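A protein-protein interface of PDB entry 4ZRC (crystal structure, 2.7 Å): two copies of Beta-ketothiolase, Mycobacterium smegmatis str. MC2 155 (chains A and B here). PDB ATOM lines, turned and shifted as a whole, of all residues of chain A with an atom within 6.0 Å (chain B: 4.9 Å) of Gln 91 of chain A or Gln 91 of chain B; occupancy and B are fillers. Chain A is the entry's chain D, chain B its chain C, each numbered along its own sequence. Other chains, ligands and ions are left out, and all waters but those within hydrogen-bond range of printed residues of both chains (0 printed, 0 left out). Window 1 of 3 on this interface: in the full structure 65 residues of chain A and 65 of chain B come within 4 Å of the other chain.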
ATOM      1  N   VAL A  59      -1.714 -21.703 -21.365  1.00  0.00           N
ATOM      2  CA  VAL A  59      -2.791 -22.010 -20.438  1.00  0.00           C
ATOM      3  C   VAL A  59      -3.708 -23.092 -21.017  1.00  0.00           C
ATOM      4  O   VAL A  59      -4.461 -22.814 -21.965  1.00  0.00           O
ATOM      5  CB  VAL A  59      -3.600 -20.771 -20.001  1.00  0.00           C
ATOM      6  CG1 VAL A  59      -4.607 -21.158 -18.913  1.00  0.00           C
ATOM      7  CG2 VAL A  59      -2.667 -19.705 -19.467  1.00  0.00           C
ATOM      8  N   ILE A  60      -3.600 -24.310 -20.461  1.00  0.00           N
ATOM      9  CA  ILE A  60      -4.356 -25.508 -20.905  1.00  0.00           C
ATOM     10  C   ILE A  60      -5.439 -25.901 -19.874  1.00  0.00           C
ATOM     11  O   ILE A  60      -5.176 -26.348 -18.740  1.00  0.00           O
ATOM     12  CB  ILE A  60      -3.449 -26.724 -21.243  1.00  0.00           C
ATOM     13  CG1 ILE A  60      -2.247 -26.325 -22.095  1.00  0.00           C
ATOM     14  CG2 ILE A  60      -4.249 -27.802 -21.943  1.00  0.00           C
ATOM     15  CD1 ILE A  60      -0.978 -27.102 -21.791  1.00  0.00           C
ATOM     16  N   LEU A  61      -6.674 -25.718 -20.304  1.00  0.00           N
ATOM     17  CA  LEU A  61      -7.803 -25.902 -19.426  1.00  0.00           C
ATOM     18  C   LEU A  61      -8.772 -26.971 -19.950  1.00  0.00           C
ATOM     19  O   LEU A  61      -9.192 -26.914 -21.110  1.00  0.00           O
ATOM     20  CB  LEU A  61      -8.515 -24.554 -19.240  1.00  0.00           C
ATOM     21  CG  LEU A  61      -8.149 -23.572 -18.133  1.00  0.00           C
ATOM     22  CD1 LEU A  61      -6.723 -23.125 -18.059  1.00  0.00           C
ATOM     23  CD2 LEU A  61      -8.924 -22.310 -18.318  1.00  0.00           C
ATOM     24  N   GLY A  62      -9.090 -27.941 -19.106  1.00  0.00           N
ATOM     25  CA  GLY A  62     -10.186 -28.833 -19.339  1.00  0.00           C
ATOM     26  C   GLY A  62     -11.440 -28.120 -18.924  1.00  0.00           C
ATOM     27  O   GLY A  62     -11.471 -27.469 -17.860  1.00  0.00           O
ATOM     28  N   HIS A  63     -12.466 -28.285 -19.767  1.00  0.00           N
ATOM     29  CA  HIS A  63     -13.713 -27.481 -19.791  1.00  0.00           C
ATOM     30  C   HIS A  63     -14.781 -28.266 -20.623  1.00  0.00           C
ATOM     31  O   HIS A  63     -14.595 -28.506 -21.798  1.00  0.00           O
ATOM     32  CB  HIS A  63     -13.373 -26.092 -20.335  1.00  0.00           C
ATOM     33  CG  HIS A  63     -14.540 -25.163 -20.469  1.00  0.00           C
ATOM     34  ND1 HIS A  63     -15.393 -24.864 -19.428  1.00  0.00           N
ATOM     35  CD2 HIS A  63     -14.963 -24.421 -21.527  1.00  0.00           C
ATOM     36  CE1 HIS A  63     -16.326 -24.033 -19.855  1.00  0.00           C
ATOM     37  NE2 HIS A  63     -16.078 -23.737 -21.120  1.00  0.00           N
ATOM     38  N   CYS A  64     -15.861 -28.700 -19.986  1.00  0.00           N
ATOM     39  CA  CYS A  64     -16.719 -29.733 -20.543  1.00  0.00           C
ATOM     40  C   CYS A  64     -18.034 -29.270 -21.172  1.00  0.00           C
ATOM     41  O   CYS A  64     -18.679 -30.011 -21.867  1.00  0.00           O
ATOM     42  CB  CYS A  64     -16.984 -30.781 -19.485  1.00  0.00           C
ATOM     43  SG  CYS A  64     -15.461 -31.584 -19.032  1.00  0.00           S
ATOM     44  N   PRO A  66     -18.361 -26.191 -23.114  1.00  0.00           N
ATOM     45  CA  PRO A  66     -17.943 -24.937 -23.737  1.00  0.00           C
ATOM     46  C   PRO A  66     -19.029 -24.355 -24.636  1.00  0.00           C
ATOM     47  O   PRO A  66     -19.935 -25.061 -25.093  1.00  0.00           O
ATOM     48  CB  PRO A  66     -16.723 -25.352 -24.574  1.00  0.00           C
ATOM     49  CG  PRO A  66     -16.882 -26.821 -24.789  1.00  0.00           C
ATOM     50  CD  PRO A  66     -17.585 -27.351 -23.605  1.00  0.00           C
ATOM     51  N   PRO A  71     -14.510 -19.142 -26.370  1.00  0.00           N
ATOM     52  CA  PRO A  71     -13.764 -20.071 -27.241  1.00  0.00           C
ATOM     53  C   PRO A  71     -12.296 -20.197 -26.854  1.00  0.00           C
ATOM     54  O   PRO A  71     -11.684 -19.236 -26.378  1.00  0.00           O
ATOM     55  CB  PRO A  71     -13.856 -19.448 -28.623  1.00  0.00           C
ATOM     56  CG  PRO A  71     -14.721 -18.249 -28.513  1.00  0.00           C
ATOM     57  CD  PRO A  71     -14.875 -17.896 -27.059  1.00  0.00           C
ATOM     58  N   ALA A  72     -11.726 -21.374 -27.111  1.00  0.00           N
ATOM     59  CA  ALA A  72     -10.392 -21.770 -26.629  1.00  0.00           C
ATOM     60  C   ALA A  72     -10.116 -21.243 -25.188  1.00  0.00           C
ATOM     61  O   ALA A  72      -9.086 -20.597 -24.919  1.00  0.00           O
ATOM     62  CB  ALA A  72      -9.317 -21.366 -27.629  1.00  0.00           C
ATOM     63  N   ILE A  73     -11.051 -21.579 -24.282  1.00  0.00           N
ATOM     64  CA  ILE A  73     -11.163 -20.991 -22.913  1.00  0.00           C
ATOM     65  C   ILE A  73      -9.859 -20.624 -22.146  1.00  0.00           C
ATOM     66  O   ILE A  73      -9.882 -19.725 -21.340  1.00  0.00           O
ATOM     67  CB  ILE A  73     -12.170 -21.765 -21.990  1.00  0.00           C
ATOM     68  CG1 ILE A  73     -12.516 -20.916 -20.770  1.00  0.00           C
ATOM     69  CG2 ILE A  73     -11.612 -23.095 -21.545  1.00  0.00           C
ATOM     70  CD1 ILE A  73     -13.790 -21.264 -20.054  1.00  0.00           C
ATOM     71  N   GLY A  74      -8.741 -21.295 -22.424  1.00  0.00           N
ATOM     72  CA  GLY A  74      -7.472 -21.077 -21.717  1.00  0.00           C
ATOM     73  C   GLY A  74      -6.811 -19.763 -22.084  1.00  0.00           C
ATOM     74  O   GLY A  74      -6.170 -19.107 -21.275  1.00  0.00           O
ATOM     75  N   GLY A  89      -3.172 -20.103 -25.215  1.00  0.00           N
ATOM     76  CA  GLY A  89      -4.132 -20.879 -24.413  1.00  0.00           C
ATOM     77  C   GLY A  89      -5.038 -21.789 -25.230  1.00  0.00           C
ATOM     78  O   GLY A  89      -5.135 -21.644 -26.448  1.00  0.00           O
ATOM     79  N   MET A  90      -5.696 -22.745 -24.563  1.00  0.00           N
ATOM     80  CA  MET A  90      -6.620 -23.649 -25.247  1.00  0.00           C
ATOM     81  C   MET A  90      -7.562 -24.381 -24.330  1.00  0.00           C
ATOM     82  O   MET A  90      -7.465 -24.286 -23.114  1.00  0.00           O
ATOM     83  CB  MET A  90      -5.862 -24.644 -26.119  1.00  0.00           C
ATOM     84  CG  MET A  90      -4.866 -25.512 -25.372  1.00  0.00           C
ATOM     85  SD  MET A  90      -4.138 -26.795 -26.377  1.00  0.00           S
ATOM     86  CE  MET A  90      -5.503 -27.933 -26.639  1.00  0.00           C
ATOM     87  N   GLN A  91      -8.474 -25.129 -24.951  1.00  0.00           N
ATOM     88  CA  GLN A  91      -9.486 -25.902 -24.241  1.00  0.00           C
ATOM     89  C   GLN A  91      -9.401 -27.404 -24.546  1.00  0.00           C
ATOM     90  O   GLN A  91      -9.261 -27.799 -25.719  1.00  0.00           O
ATOM     91  CB  GLN A  91     -10.876 -25.360 -24.546  1.00  0.00           C
ATOM     92  CG  GLN A  91     -12.031 -26.181 -23.934  1.00  0.00           C
ATOM     93  CD  GLN A  91     -12.688 -27.159 -24.905  1.00  0.00           C
ATOM     94  OE1 GLN A  91     -12.657 -26.974 -26.130  1.00  0.00           O
ATOM     95  NE2 GLN A  91     -13.292 -28.178 -24.360  1.00  0.00           N
ATOM     96  N   VAL A  92      -9.487 -28.237 -23.493  1.00  0.00           N
ATOM     97  CA  VAL A  92      -9.638 -29.702 -23.675  1.00  0.00           C
ATOM     98  C   VAL A  92     -10.920 -30.273 -23.081  1.00  0.00           C
ATOM     99  O   VAL A  92     -11.435 -29.759 -22.077  1.00  0.00           O
ATOM    100  CB  VAL A  92      -8.410 -30.526 -23.209  1.00  0.00           C
ATOM    101  CG1 VAL A  92      -7.179 -30.112 -24.035  1.00  0.00           C
ATOM    102  CG2 VAL A  92      -8.208 -30.453 -21.684  1.00  0.00           C
ATOM    103  N   ASP A  93     -11.416 -31.329 -23.737  1.00  0.00           N
ATOM    104  CA  ASP A  93     -12.558 -32.124 -23.259  1.00  0.00           C
ATOM    105  C   ASP A  93     -12.312 -33.645 -23.366  1.00  0.00           C
ATOM    106  O   ASP A  93     -12.308 -34.238 -24.420  1.00  0.00           O
ATOM    107  CB  ASP A  93     -13.870 -31.671 -23.970  1.00  0.00           C
ATOM    108  CG  ASP A  93     -15.131 -32.404 -23.492  1.00  0.00           C
ATOM    109  OD1 ASP A  93     -15.197 -32.953 -22.378  1.00  0.00           O
ATOM    110  OD2 ASP A  93     -16.086 -32.429 -24.284  1.00  0.00           O
ATOM    111  N   ARG A  94     -12.076 -34.251 -22.232  1.00  0.00           N
ATOM    112  CA  ARG A  94     -12.251 -35.685 -22.059  1.00  0.00           C
ATOM    113  C   ARG A  94     -13.147 -35.913 -20.806  1.00  0.00           C
ATOM    114  O   ARG A  94     -12.775 -36.595 -19.841  1.00  0.00           O
ATOM    115  CB  ARG A  94     -10.890 -36.392 -21.979  1.00  0.00           C
ATOM    116  CG  ARG A  94     -11.006 -37.883 -21.963  1.00  0.00           C
ATOM    117  CD  ARG A  94      -9.648 -38.548 -21.929  1.00  0.00           C
ATOM    118  NE  ARG A  94      -9.346 -39.180 -23.199  1.00  0.00           N
ATOM    119  CZ  ARG A  94      -8.203 -39.062 -23.837  1.00  0.00           C
ATOM    120  NH1 ARG A  94      -7.199 -38.400 -23.325  1.00  0.00           N
ATOM    121  NH2 ARG A  94      -8.076 -39.644 -24.997  1.00  0.00           N
ATOM    122  N   LEU B  61      -9.474 -35.161 -31.589  1.00  0.00           N
ATOM    123  CA  LEU B  61     -10.067 -34.288 -32.596  1.00  0.00           C
ATOM    124  C   LEU B  61     -10.173 -32.817 -32.176  1.00  0.00           C
ATOM    125  O   LEU B  61     -10.660 -32.505 -31.078  1.00  0.00           O
ATOM    126  CB  LEU B  61     -11.452 -34.810 -32.973  1.00  0.00           C
ATOM    127  CG  LEU B  61     -11.673 -35.875 -34.062  1.00  0.00           C
ATOM    128  CD1 LEU B  61     -10.863 -37.109 -33.969  1.00  0.00           C
ATOM    129  CD2 LEU B  61     -13.111 -36.313 -34.078  1.00  0.00           C
ATOM    130  N   HIS B  63     -12.049 -29.362 -32.761  1.00  0.00           N
ATOM    131  CA  HIS B  63     -13.475 -29.171 -32.952  1.00  0.00           C
ATOM    132  C   HIS B  63     -13.845 -27.887 -32.231  1.00  0.00           C
ATOM    133  O   HIS B  63     -13.725 -27.780 -31.026  1.00  0.00           O
ATOM    134  CB  HIS B  63     -14.206 -30.443 -32.448  1.00  0.00           C
ATOM    135  CG  HIS B  63     -15.699 -30.371 -32.471  1.00  0.00           C
ATOM    136  ND1 HIS B  63     -16.420 -30.109 -33.611  1.00  0.00           N
ATOM    137  CD2 HIS B  63     -16.608 -30.547 -31.486  1.00  0.00           C
ATOM    138  CE1 HIS B  63     -17.707 -30.108 -33.331  1.00  0.00           C
ATOM    139  NE2 HIS B  63     -17.850 -30.381 -32.051  1.00  0.00           N
ATOM    140  N   PRO B  66     -18.209 -27.057 -30.287  1.00  0.00           N
ATOM    141  CA  PRO B  66     -18.807 -28.218 -29.637  1.00  0.00           C
ATOM    142  C   PRO B  66     -20.132 -27.938 -28.933  1.00  0.00           C
ATOM    143  O   PRO B  66     -20.481 -26.829 -28.673  1.00  0.00           O
ATOM    144  CB  PRO B  66     -17.719 -28.682 -28.639  1.00  0.00           C
ATOM    145  CG  PRO B  66     -16.864 -27.494 -28.404  1.00  0.00           C
ATOM    146  CD  PRO B  66     -16.910 -26.701 -29.676  1.00  0.00           C
ATOM    147  N   ALA B  72     -16.921 -34.799 -25.649  1.00  0.00           N
ATOM    148  CA  ALA B  72     -15.617 -35.445 -25.946  1.00  0.00           C
ATOM    149  C   ALA B  72     -15.557 -36.061 -27.372  1.00  0.00           C
ATOM    150  O   ALA B  72     -15.188 -37.202 -27.507  1.00  0.00           O
ATOM    151  CB  ALA B  72     -15.253 -36.471 -24.861  1.00  0.00           C
ATOM    152  N   ILE B  73     -15.897 -35.260 -28.392  1.00  0.00           N
ATOM    153  CA  ILE B  73     -16.197 -35.695 -29.786  1.00  0.00           C
ATOM    154  C   ILE B  73     -15.361 -36.840 -30.417  1.00  0.00           C
ATOM    155  O   ILE B  73     -15.874 -37.551 -31.247  1.00  0.00           O
ATOM    156  CB  ILE B  73     -16.336 -34.474 -30.780  1.00  0.00           C
ATOM    157  CG1 ILE B  73     -17.072 -34.900 -32.055  1.00  0.00           C
ATOM    158  CG2 ILE B  73     -14.971 -33.855 -31.086  1.00  0.00           C
ATOM    159  CD1 ILE B  73     -17.497 -33.837 -33.009  1.00  0.00           C
ATOM    160  N   GLY B  74     -14.108 -37.022 -30.008  1.00  0.00           N
ATOM    161  CA  GLY B  74     -13.229 -38.083 -30.517  1.00  0.00           C
ATOM    162  C   GLY B  74     -13.646 -39.482 -30.091  1.00  0.00           C
ATOM    163  O   GLY B  74     -13.569 -40.445 -30.824  1.00  0.00           O
ATOM    164  N   GLY B  89     -10.953 -41.366 -26.518  1.00  0.00           N
ATOM    165  CA  GLY B  89     -11.010 -40.203 -27.369  1.00  0.00           C
ATOM    166  C   GLY B  89     -11.353 -38.908 -26.670  1.00  0.00           C
ATOM    167  O   GLY B  89     -11.795 -38.899 -25.528  1.00  0.00           O
ATOM    168  N   MET B  90     -11.140 -37.807 -27.387  1.00  0.00           N
ATOM    169  CA  MET B  90     -11.316 -36.479 -26.816  1.00  0.00           C
ATOM    170  C   MET B  90     -11.479 -35.366 -27.854  1.00  0.00           C
ATOM    171  O   MET B  90     -11.422 -35.589 -29.052  1.00  0.00           O
ATOM    172  CB  MET B  90     -10.233 -36.154 -25.779  1.00  0.00           C
ATOM    173  CG  MET B  90      -8.812 -36.232 -26.305  1.00  0.00           C
ATOM    174  SD  MET B  90      -7.491 -35.530 -25.290  1.00  0.00           S
ATOM    175  CE  MET B  90      -7.913 -33.808 -25.238  1.00  0.00           C
ATOM    176  N   GLN B  91     -11.697 -34.159 -27.333  1.00  0.00           N
ATOM    177  CA  GLN B  91     -11.894 -32.933 -28.104  1.00  0.00           C
ATOM    178  C   GLN B  91     -10.891 -31.843 -27.657  1.00  0.00           C
ATOM    179  O   GLN B  91     -10.656 -31.640 -26.451  1.00  0.00           O
ATOM    180  CB  GLN B  91     -13.353 -32.456 -27.954  1.00  0.00           C
ATOM    181  CG  GLN B  91     -13.697 -31.156 -28.662  1.00  0.00           C
ATOM    182  CD  GLN B  91     -13.602 -29.934 -27.786  1.00  0.00           C
ATOM    183  OE1 GLN B  91     -13.871 -29.980 -26.600  1.00  0.00           O
ATOM    184  NE2 GLN B  91     -13.280 -28.829 -28.382  1.00  0.00           N
ATOM    185  N   VAL B  92     -10.297 -31.166 -28.642  1.00  0.00           N
ATOM    186  CA  VAL B  92      -9.467 -29.984 -28.414  1.00  0.00           C
ATOM    187  C   VAL B  92      -9.958 -28.768 -29.169  1.00  0.00           C
ATOM    188  O   VAL B  92     -10.470 -28.893 -30.278  1.00  0.00           O
ATOM    189  CB  VAL B  92      -7.953 -30.182 -28.699  1.00  0.00           C
ATOM    190  CG1 VAL B  92      -7.340 -31.199 -27.747  1.00  0.00           C
ATOM    191  CG2 VAL B  92      -7.639 -30.448 -30.185  1.00  0.00           C
ATOM    192  N   ASP B  93      -9.808 -27.603 -28.522  1.00  0.00           N
ATOM    193  CA  ASP B  93     -10.077 -26.293 -29.091  1.00  0.00           C
ATOM    194  C   ASP B  93      -8.922 -25.325 -28.873  1.00  0.00           C
ATOM    195  O   ASP B  93      -8.675 -24.865 -27.780  1.00  0.00           O
ATOM    196  CB  ASP B  93     -11.377 -25.708 -28.526  1.00  0.00           C
ATOM    197  CG  ASP B  93     -11.796 -24.378 -29.210  1.00  0.00           C
ATOM    198  OD1 ASP B  93     -11.392 -24.093 -30.352  1.00  0.00           O
ATOM    199  OD2 ASP B  93     -12.544 -23.612 -28.569  1.00  0.00           O
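Of the printed residues of chain B, Ala 72 of chain A touches Asp 93 (2.8 Å). Of chain B, only Gln 91 (2.9 Å), Val 92 (3.5 Å) and Asp 93 (2.8 Å) come within 4 Å of Gln 91 of chain A. Of the printed residues of chain B, Val 92 of chain A touches Met 90, Gln 91 and Val 92. Printed residues of chain B within 4 Å of Asp 93 of chain A: Ala 72 (2.9 Å), Met 90 (3.1 Å) and Gln 91 (2.8 Å). Of chain A, only Gln 91 (2.9 Å), Val 92 (3.5 Å) and Asp 93 (2.8 Å) come within 4 Å of Gln 91 of chain B. The nearest residue of chain B that does not touch Gln 91 of chain A is Pro 66 of chain B (4.8 Å). The nearest residue of chain A that does not touch Gln 91 of chain B is Pro 66 of chain A (4.7 Å).
Ala 72 of chain A touches Asp 93 of chain B, and with the chains exchanged Asp 93 of chain A touches Ala 72 of chain B. Gln 91 of chain B touches its own counterpart, Gln 91 of chain A. Gln 91 of chain A touches Val 92 of chain B, and with the chains exchanged Val 92 of chain A touches Gln 91 of chain B. Val 92 of chain B touches its own counterpart, Val 92 of chain A. Of the 16 pairs that touch across the chains among the printed residues, 13 have their exchanged pair printed and touching as well.
CG of Pro 66 of chain A touches CG of Pro 66 of chain B, at 3.7 Å. Asp 93 of chain B touches Pro 71 of chain A. Met 90 of chain A touches Val 92 of chain B. Met 90 of chain A touches Asp 93 of chain B (CB to O, 3.3 Å). Val 92 of chain B touches Gln 91 of chain A (CA to O, 3.5 Å). CE of Met 90 of chain B touches CB of Val 92 of chain A (3.9 Å). Gln 91 of chain B touches Val 92 of chain A. Val 92 of chain A touches Val 92 of chain B (CG1 to CG1, 3.9 Å). O of Asp 93 of chain A touches CB of Met 90 of chain B, at 3.1 Å.
Hydrophobic or aromatic side chains of chain A that line the printed part of chain B: Pro 66, Ala 72, Met 90 and Val 92.
The side-chain carboxylate of Asp 93 of chain A lies within hydrogen-bond range of the backbone NH of Ala 72 of chain B (2.9 Å). NE of Arg 94 of chain A lies within hydrogen-bond range of O of Gly 89 of chain B. The side-chain sulfur (SD) of Met 90 of chain B sits at hydrogen-bond distance from the guanidinium group (NH1) of Arg 94 of chain A (3.5 Å). The side-chain amide oxygen of Gln 91 of chain B is in hydrogen-bond range of the side-chain amide nitrogen of Gln 91 of chain A, 2.9 Å away. The backbone carbonyl oxygen (O) of Gln 91 of chain B sits at hydrogen-bond distance from the backbone NH (N) of Asp 93 of chain A, at 2.8 Å. The side-chain carboxylate of Asp 93 of chain B sits at hydrogen-bond distance from the backbone NH of Ala 72 of chain A, 2.8 Å away. The backbone carbonyl oxygen (O) of Asp 93 of chain B sits at hydrogen-bond distance from the backbone NH (N) of Gln 91 of chain A, 2.8 Å away.
O of Leu 61 of chain B sits at hydrogen-bond distance from N of Val 92 of chain B (2.8 Å). The side-chain amide nitrogen (NE2) of Gln 91 of chain B lies within hydrogen-bond range of the backbone carbonyl oxygen (O) of His 63 of chain B, 2.9 Å away. The backbone NH (N) of His 63 of chain B lies within hydrogen-bond range of the backbone carbonyl oxygen (O) of Val 92 of chain B. The backbone carbonyl oxygen of Met 90 of chain B is in hydrogen-bond range of the backbone NH of Gly 74 of chain B (3.2 Å). The backbone carbonyl oxygen (O) of Val 59 of chain A is in hydrogen-bond range of the backbone NH (N) of Met 90 of chain A (2.9 Å). SG of Cys 64 of chain A lies within hydrogen-bond range of OD1 of Asp 93 of chain A, 3.6 Å away.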
